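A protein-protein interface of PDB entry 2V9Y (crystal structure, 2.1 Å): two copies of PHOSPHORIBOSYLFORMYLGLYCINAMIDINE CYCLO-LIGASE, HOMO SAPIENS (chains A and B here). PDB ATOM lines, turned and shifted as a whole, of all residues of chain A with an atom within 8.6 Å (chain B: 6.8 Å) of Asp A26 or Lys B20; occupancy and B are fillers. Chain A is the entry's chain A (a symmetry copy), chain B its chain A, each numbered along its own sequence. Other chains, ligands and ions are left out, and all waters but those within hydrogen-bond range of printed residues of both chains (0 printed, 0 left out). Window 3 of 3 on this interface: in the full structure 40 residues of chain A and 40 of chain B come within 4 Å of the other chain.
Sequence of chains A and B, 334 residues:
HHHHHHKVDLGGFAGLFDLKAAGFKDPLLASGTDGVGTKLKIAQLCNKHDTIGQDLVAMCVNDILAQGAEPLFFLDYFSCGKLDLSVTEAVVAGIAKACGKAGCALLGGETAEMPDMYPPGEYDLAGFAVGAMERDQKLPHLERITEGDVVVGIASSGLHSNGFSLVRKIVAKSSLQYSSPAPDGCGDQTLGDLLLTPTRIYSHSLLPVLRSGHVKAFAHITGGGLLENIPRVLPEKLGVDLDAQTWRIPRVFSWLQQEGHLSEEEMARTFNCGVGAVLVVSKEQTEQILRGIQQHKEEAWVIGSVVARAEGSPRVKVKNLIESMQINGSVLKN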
ATOM      1  N   LEU A  19     -10.724 -25.482  -0.631  1.00  0.00           N
ATOM      2  CA  LEU A  19      -9.513 -25.383  -1.477  1.00  0.00           C
ATOM      3  C   LEU A  19      -9.376 -26.563  -2.428  1.00  0.00           C
ATOM      4  O   LEU A  19      -8.883 -26.403  -3.537  1.00  0.00           O
ATOM      5  CB  LEU A  19      -8.231 -25.275  -0.641  1.00  0.00           C
ATOM      6  CG  LEU A  19      -7.939 -23.973   0.114  1.00  0.00           C
ATOM      7  CD1 LEU A  19      -7.000 -24.258   1.288  1.00  0.00           C
ATOM      8  CD2 LEU A  19      -7.392 -22.916  -0.793  1.00  0.00           C
ATOM      9  N   GLY A  23      -9.253 -26.872  -6.571  1.00  0.00           N
ATOM     10  CA  GLY A  23      -8.215 -27.514  -7.387  1.00  0.00           C
ATOM     11  C   GLY A  23      -6.775 -27.247  -6.991  1.00  0.00           C
ATOM     12  O   GLY A  23      -5.869 -27.435  -7.797  1.00  0.00           O
ATOM     13  N   PHE A  24      -6.549 -26.819  -5.754  1.00  0.00           N
ATOM     14  CA  PHE A  24      -5.180 -26.646  -5.261  1.00  0.00           C
ATOM     15  C   PHE A  24      -4.597 -27.971  -4.768  1.00  0.00           C
ATOM     16  O   PHE A  24      -5.286 -28.759  -4.122  1.00  0.00           O
ATOM     17  CB  PHE A  24      -5.122 -25.532  -4.200  1.00  0.00           C
ATOM     18  CG  PHE A  24      -5.375 -24.157  -4.777  1.00  0.00           C
ATOM     19  CD1 PHE A  24      -6.662 -23.615  -4.785  1.00  0.00           C
ATOM     20  CD2 PHE A  24      -4.334 -23.431  -5.352  1.00  0.00           C
ATOM     21  CE1 PHE A  24      -6.891 -22.375  -5.336  1.00  0.00           C
ATOM     22  CE2 PHE A  24      -4.555 -22.184  -5.913  1.00  0.00           C
ATOM     23  CZ  PHE A  24      -5.838 -21.651  -5.911  1.00  0.00           C
ATOM     24  N   LYS A  25      -3.343 -28.243  -5.132  1.00  0.00           N
ATOM     25  CA  LYS A  25      -2.656 -29.439  -4.650  1.00  0.00           C
ATOM     26  C   LYS A  25      -1.941 -29.114  -3.334  1.00  0.00           C
ATOM     27  O   LYS A  25      -2.164 -29.759  -2.314  1.00  0.00           O
ATOM     28  CB  LYS A  25      -1.670 -29.975  -5.695  1.00  0.00           C
ATOM     29  CG  LYS A  25      -2.228 -30.115  -7.111  1.00  0.00           C
ATOM     30  CD  LYS A  25      -1.885 -31.506  -7.683  1.00  0.00           C
ATOM     31  CE  LYS A  25      -1.251 -31.428  -9.083  1.00  0.00           C
ATOM     32  NZ  LYS A  25      -0.486 -32.672  -9.382  1.00  0.00           N
ATOM     33  N   ASP A  26      -1.109 -28.075  -3.372  1.00  0.00           N
ATOM     34  CA  ASP A  26      -0.278 -27.682  -2.234  1.00  0.00           C
ATOM     35  C   ASP A  26      -0.259 -26.141  -2.112  1.00  0.00           C
ATOM     36  O   ASP A  26       0.721 -25.498  -2.492  1.00  0.00           O
ATOM     37  CB  ASP A  26       1.132 -28.249  -2.463  1.00  0.00           C
ATOM     38  CG  ASP A  26       2.020 -28.182  -1.231  1.00  0.00           C
ATOM     39  OD1 ASP A  26       1.521 -27.986  -0.090  1.00  0.00           O
ATOM     40  OD2 ASP A  26       3.251 -28.327  -1.429  1.00  0.00           O
ATOM     41  N   PRO A  27      -1.355 -25.541  -1.598  1.00  0.00           N
ATOM     42  CA  PRO A  27      -1.444 -24.068  -1.668  1.00  0.00           C
ATOM     43  C   PRO A  27      -0.705 -23.342  -0.549  1.00  0.00           C
ATOM     44  O   PRO A  27      -0.615 -23.854   0.564  1.00  0.00           O
ATOM     45  CB  PRO A  27      -2.955 -23.796  -1.545  1.00  0.00           C
ATOM     46  CG  PRO A  27      -3.475 -24.985  -0.759  1.00  0.00           C
ATOM     47  CD  PRO A  27      -2.537 -26.148  -0.959  1.00  0.00           C
ATOM     48  N   LEU A  28      -0.181 -22.159  -0.857  1.00  0.00           N
ATOM     49  CA  LEU A  28       0.107 -21.153   0.169  1.00  0.00           C
ATOM     50  C   LEU A  28      -1.004 -20.139   0.097  1.00  0.00           C
ATOM     51  O   LEU A  28      -1.542 -19.892  -0.985  1.00  0.00           O
ATOM     52  CB  LEU A  28       1.438 -20.433  -0.075  1.00  0.00           C
ATOM     53  CG  LEU A  28       2.724 -21.253  -0.155  1.00  0.00           C
ATOM     54  CD1 LEU A  28       3.867 -20.312  -0.496  1.00  0.00           C
ATOM     55  CD2 LEU A  28       2.982 -22.002   1.139  1.00  0.00           C
ATOM     56  N   LEU A  29      -1.339 -19.537   1.238  1.00  0.00           N
ATOM     57  CA  LEU A  29      -2.385 -18.502   1.283  1.00  0.00           C
ATOM     58  C   LEU A  29      -1.789 -17.110   1.412  1.00  0.00           C
ATOM     59  O   LEU A  29      -0.943 -16.883   2.282  1.00  0.00           O
ATOM     60  CB  LEU A  29      -3.350 -18.760   2.452  1.00  0.00           C
ATOM     61  CG  LEU A  29      -4.117 -20.089   2.544  1.00  0.00           C
ATOM     62  CD1 LEU A  29      -4.857 -20.155   3.879  1.00  0.00           C
ATOM     63  CD2 LEU A  29      -5.080 -20.260   1.368  1.00  0.00           C
ATOM     64  N   ALA A 132      -4.533 -17.744  -3.154  1.00  0.00           N
ATOM     65  CA  ALA A 132      -3.763 -18.974  -3.028  1.00  0.00           C
ATOM     66  C   ALA A 132      -2.987 -19.208  -4.310  1.00  0.00           C
ATOM     67  O   ALA A 132      -3.373 -18.750  -5.390  1.00  0.00           O
ATOM     68  CB  ALA A 132      -4.663 -20.155  -2.733  1.00  0.00           C
ATOM     69  N   MET A 133      -1.869 -19.891  -4.170  1.00  0.00           N
ATOM     70  CA  MET A 133      -1.094 -20.337  -5.310  1.00  0.00           C
ATOM     71  C   MET A 133      -0.295 -21.531  -4.849  1.00  0.00           C
ATOM     72  O   MET A 133      -0.228 -21.809  -3.646  1.00  0.00           O
ATOM     73  CB  MET A 133      -0.196 -19.210  -5.869  1.00  0.00           C
ATOM     74  CG  MET A 133       1.142 -19.000  -5.174  1.00  0.00           C
ATOM     75  SD  MET A 133       0.948 -18.442  -3.491  1.00  0.00           S
ATOM     76  CE  MET A 133       1.586 -16.786  -3.544  1.00  0.00           C
ATOM     77  N   GLU A 134       0.283 -22.251  -5.808  1.00  0.00           N
ATOM     78  CA  GLU A 134       1.245 -23.313  -5.511  1.00  0.00           C
ATOM     79  C   GLU A 134       2.500 -22.758  -4.853  1.00  0.00           C
ATOM     80  O   GLU A 134       2.879 -21.617  -5.078  1.00  0.00           O
ATOM     81  CB  GLU A 134       1.614 -24.087  -6.787  1.00  0.00           C
ATOM     82  CG  GLU A 134       1.102 -25.503  -6.818  1.00  0.00           C
ATOM     83  CD  GLU A 134      -0.399 -25.615  -6.699  1.00  0.00           C
ATOM     84  OE1 GLU A 134      -1.071 -25.011  -7.550  1.00  0.00           O
ATOM     85  OE2 GLU A 134      -0.893 -26.332  -5.791  1.00  0.00           O
ATOM     86  N   ARG A 135       3.142 -23.580  -4.040  1.00  0.00           N
ATOM     87  CA  ARG A 135       4.388 -23.205  -3.391  1.00  0.00           C
ATOM     88  C   ARG A 135       5.419 -22.625  -4.389  1.00  0.00           C
ATOM     89  O   ARG A 135       6.057 -21.609  -4.076  1.00  0.00           O
ATOM     90  CB  ARG A 135       4.928 -24.400  -2.580  1.00  0.00           C
ATOM     91  CG  ARG A 135       6.158 -24.097  -1.751  1.00  0.00           C
ATOM     92  CD  ARG A 135       6.517 -25.253  -0.812  1.00  0.00           C
ATOM     93  NE  ARG A 135       5.843 -25.133   0.488  1.00  0.00           N
ATOM     94  CZ  ARG A 135       4.749 -25.808   0.819  1.00  0.00           C
ATOM     95  NH1 ARG A 135       4.210 -26.640  -0.049  1.00  0.00           N
ATOM     96  NH2 ARG A 135       4.197 -25.659   1.998  1.00  0.00           N
ATOM     97  N   ASP A 136       5.550 -23.231  -5.583  1.00  0.00           N
ATOM     98  CA  ASP A 136       6.473 -22.729  -6.647  1.00  0.00           C
ATOM     99  C   ASP A 136       5.988 -21.507  -7.453  1.00  0.00           C
ATOM    100  O   ASP A 136       6.805 -20.796  -8.063  1.00  0.00           O
ATOM    101  CB  ASP A 136       6.952 -23.857  -7.598  1.00  0.00           C
ATOM    102  CG  ASP A 136       5.802 -24.571  -8.334  1.00  0.00           C
ATOM    103  OD1 ASP A 136       4.769 -23.942  -8.652  1.00  0.00           O
ATOM    104  OD2 ASP A 136       5.945 -25.777  -8.612  1.00  0.00           O
ATOM    105  N   GLN A 137       4.674 -21.241  -7.413  1.00  0.00           N
ATOM    106  CA  GLN A 137       4.062 -20.097  -8.108  1.00  0.00           C
ATOM    107  C   GLN A 137       4.195 -18.769  -7.352  1.00  0.00           C
ATOM    108  O   GLN A 137       3.685 -17.739  -7.791  1.00  0.00           O
ATOM    109  CB  GLN A 137       2.581 -20.393  -8.402  1.00  0.00           C
ATOM    110  CG  GLN A 137       2.327 -21.343  -9.571  1.00  0.00           C
ATOM    111  CD  GLN A 137       0.917 -21.932  -9.562  1.00  0.00           C
ATOM    112  OE1 GLN A 137       0.136 -21.720  -8.627  1.00  0.00           O
ATOM    113  NE2 GLN A 137       0.589 -22.686 -10.610  1.00  0.00           N
ATOM    114  N   PHE B  17       0.540 -17.826   4.439  1.00  0.00           N
ATOM    115  CA  PHE B  17       0.268 -18.922   5.350  1.00  0.00           C
ATOM    116  C   PHE B  17       0.422 -20.297   4.688  1.00  0.00           C
ATOM    117  O   PHE B  17      -0.043 -20.524   3.567  1.00  0.00           O
ATOM    118  CB  PHE B  17      -1.098 -18.732   6.056  1.00  0.00           C
ATOM    119  CG  PHE B  17      -1.216 -19.489   7.345  1.00  0.00           C
ATOM    120  CD1 PHE B  17      -0.881 -18.894   8.544  1.00  0.00           C
ATOM    121  CD2 PHE B  17      -1.619 -20.808   7.351  1.00  0.00           C
ATOM    122  CE1 PHE B  17      -0.974 -19.621   9.742  1.00  0.00           C
ATOM    123  CE2 PHE B  17      -1.694 -21.538   8.535  1.00  0.00           C
ATOM    124  CZ  PHE B  17      -1.374 -20.938   9.727  1.00  0.00           C
ATOM    125  N   ASP B  18       1.129 -21.194   5.381  1.00  0.00           N
ATOM    126  CA  ASP B  18       1.474 -22.516   4.878  1.00  0.00           C
ATOM    127  C   ASP B  18       0.581 -23.525   5.614  1.00  0.00           C
ATOM    128  O   ASP B  18       0.872 -23.900   6.764  1.00  0.00           O
ATOM    129  CB  ASP B  18       2.977 -22.768   5.130  1.00  0.00           C
ATOM    130  CG  ASP B  18       3.503 -24.064   4.506  1.00  0.00           C
ATOM    131  OD1 ASP B  18       2.728 -24.999   4.212  1.00  0.00           O
ATOM    132  OD2 ASP B  18       4.733 -24.163   4.325  1.00  0.00           O
ATOM    133  N   LEU B  19      -0.516 -23.941   4.969  1.00  0.00           N
ATOM    134  CA  LEU B  19      -1.479 -24.876   5.594  1.00  0.00           C
ATOM    135  C   LEU B  19      -0.863 -26.239   5.872  1.00  0.00           C
ATOM    136  O   LEU B  19      -1.213 -26.882   6.853  1.00  0.00           O
ATOM    137  CB  LEU B  19      -2.736 -25.071   4.735  1.00  0.00           C
ATOM    138  CG  LEU B  19      -3.751 -23.927   4.627  1.00  0.00           C
ATOM    139  CD1 LEU B  19      -4.562 -24.079   3.338  1.00  0.00           C
ATOM    140  CD2 LEU B  19      -4.634 -23.853   5.833  1.00  0.00           C
ATOM    141  N   LYS B  20       0.046 -26.660   5.004  1.00  0.00           N
ATOM    142  CA  LYS B  20       0.741 -27.951   5.146  1.00  0.00           C
ATOM    143  C   LYS B  20       1.578 -27.965   6.424  1.00  0.00           C
ATOM    144  O   LYS B  20       1.380 -28.827   7.288  1.00  0.00           O
ATOM    145  CB  LYS B  20       1.612 -28.247   3.942  1.00  0.00           C
ATOM    146  CG  LYS B  20       1.936 -29.726   3.795  1.00  0.00           C
ATOM    147  CD  LYS B  20       2.757 -29.978   2.560  1.00  0.00           C
ATOM    148  CE  LYS B  20       2.390 -31.313   1.948  1.00  0.00           C
ATOM    149  NZ  LYS B  20       3.375 -31.754   0.922  1.00  0.00           N
ATOM    150  N   ALA B  21       2.478 -26.978   6.542  1.00  0.00           N
ATOM    151  CA  ALA B  21       3.304 -26.800   7.736  1.00  0.00           C
ATOM    152  C   ALA B  21       2.444 -26.756   8.991  1.00  0.00           C
ATOM    153  O   ALA B  21       2.830 -27.330  10.010  1.00  0.00           O
ATOM    154  CB  ALA B  21       4.190 -25.565   7.624  1.00  0.00           C
ATOM    155  N   ALA B  22       1.269 -26.124   8.892  1.00  0.00           N
ATOM    156  CA  ALA B  22       0.273 -26.104   9.961  1.00  0.00           C
ATOM    157  C   ALA B  22      -0.394 -27.451  10.251  1.00  0.00           C
ATOM    158  O   ALA B  22      -1.075 -27.584  11.260  1.00  0.00           O
ATOM    159  CB  ALA B  22      -0.797 -25.030   9.701  1.00  0.00           C
ATOM    160  N   GLY B  23      -0.248 -28.421   9.355  1.00  0.00           N
ATOM    161  CA  GLY B  23      -0.690 -29.792   9.638  1.00  0.00           C
ATOM    162  C   GLY B  23      -2.102 -30.153   9.217  1.00  0.00           C
ATOM    163  O   GLY B  23      -2.665 -31.123   9.717  1.00  0.00           O
ATOM    164  N   PHE B  24      -2.680 -29.392   8.295  1.00  0.00           N
ATOM    165  CA  PHE B  24      -3.997 -29.741   7.755  1.00  0.00           C
ATOM    166  C   PHE B  24      -3.880 -30.778   6.637  1.00  0.00           C
ATOM    167  O   PHE B  24      -2.980 -30.703   5.802  1.00  0.00           O
ATOM    168  CB  PHE B  24      -4.759 -28.476   7.324  1.00  0.00           C
ATOM    169  CG  PHE B  24      -5.170 -27.610   8.495  1.00  0.00           C
ATOM    170  CD1 PHE B  24      -4.355 -26.561   8.924  1.00  0.00           C
ATOM    171  CD2 PHE B  24      -6.347 -27.877   9.191  1.00  0.00           C
ATOM    172  CE1 PHE B  24      -4.720 -25.793  10.006  1.00  0.00           C
ATOM    173  CE2 PHE B  24      -6.722 -27.114  10.284  1.00  0.00           C
ATOM    174  CZ  PHE B  24      -5.906 -26.069  10.700  1.00  0.00           C
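The side-chain carboxylate (OD1) of Asp B18 lies within salt-bridge range of the guanidinium group (NH2) of Arg A135, at 2.7 Å. The backbone NH (N) of Phe B17 sits at hydrogen-bond distance from the backbone carbonyl oxygen (O) of Leu A29 (2.8 Å).
The backbone NH of Leu A28 lies within hydrogen-bond range of the backbone carbonyl oxygen of Met A133, 2.8 Å away. The guanidinium group of Arg A135 is in salt-bridge range of the side-chain carboxylate of Asp A26 (3.0 Å). The backbone carbonyl oxygen (O) of Leu A19 is in hydrogen-bond range of the backbone NH (N) of Phe A24, at 3.2 Å. The side-chain carboxylate (OD1) of Asp B18 is in hydrogen-bond range of the backbone NH (N) of Ala B21 (3.1 Å). The backbone NH (N) of Phe B24 is in hydrogen-bond range of the backbone carbonyl oxygen (O) of Leu B19, 3.2 Å away. OD1 of Asp B18 sits close to N of Lys B20 (3.3 Å).
CD1 of Leu A19 touches CD1 of Leu B19 (3.2 Å). Asp A26 touches Lys B20. Leu A28 touches Phe B17. CD2 of Leu A28 touches CG of Asp B18, 3.98 Å away. CD1 of Leu A29 touches CD1 of Leu B19, 3.97 Å away.
Of the printed residues of chain B, Leu A19 touches Leu B19. Of chain B, only Lys B20 (3.5 Å) comes within 4 Å of Asp A26. Printed residues of chain B within 4 Å of Leu A28: Phe B17 and Asp B18. Of the printed residues of chain B, Leu A29 touches Phe B17 (2.8 Å) and Leu B19 (3.97 Å). Ala A132 touches none of the printed residues of chain B. Gln A137 touches none of the printed residues of chain B. Printed residues of chain A within 4 Å of Phe B17: Leu A28 (3.5 Å) and Leu A29 (2.8 Å). Of the printed residues of chain A, Leu B19 touches Leu A19 and Leu A29. Lys B20 touches one residue of chain A. The nearest residue of chain B that does not touch Asp A26 is Asp B18 (5.4 Å). The nearest residue of chain A that does not touch Lys B20 is Arg A135 (4.1 Å). The nearest printed residue of chain A that does not touch Phe B17 is Pro A27 (4.5 Å).
Of the 8 printed residues of chain B, 4 touch a printed residue of chain A. Hydrophobic or aromatic side chains of chain B within 4 Å of the printed part of chain A: Leu B19. Hydrophobic or aromatic side chains of chain A that line the printed part of chain B: Leu A19, Leu A28 and Leu A29. Among the printed residues, 7 pairs touch across the chains. Among the printed residues, Asp or Glu carboxylates within 4 Å of a Lys or Arg side-chain nitrogen of the other chain: Arg A135 with Asp B18 (2.7 Å).
Leu A19 touches its own counterpart, Leu B19. 3 positions are printed for both chains.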
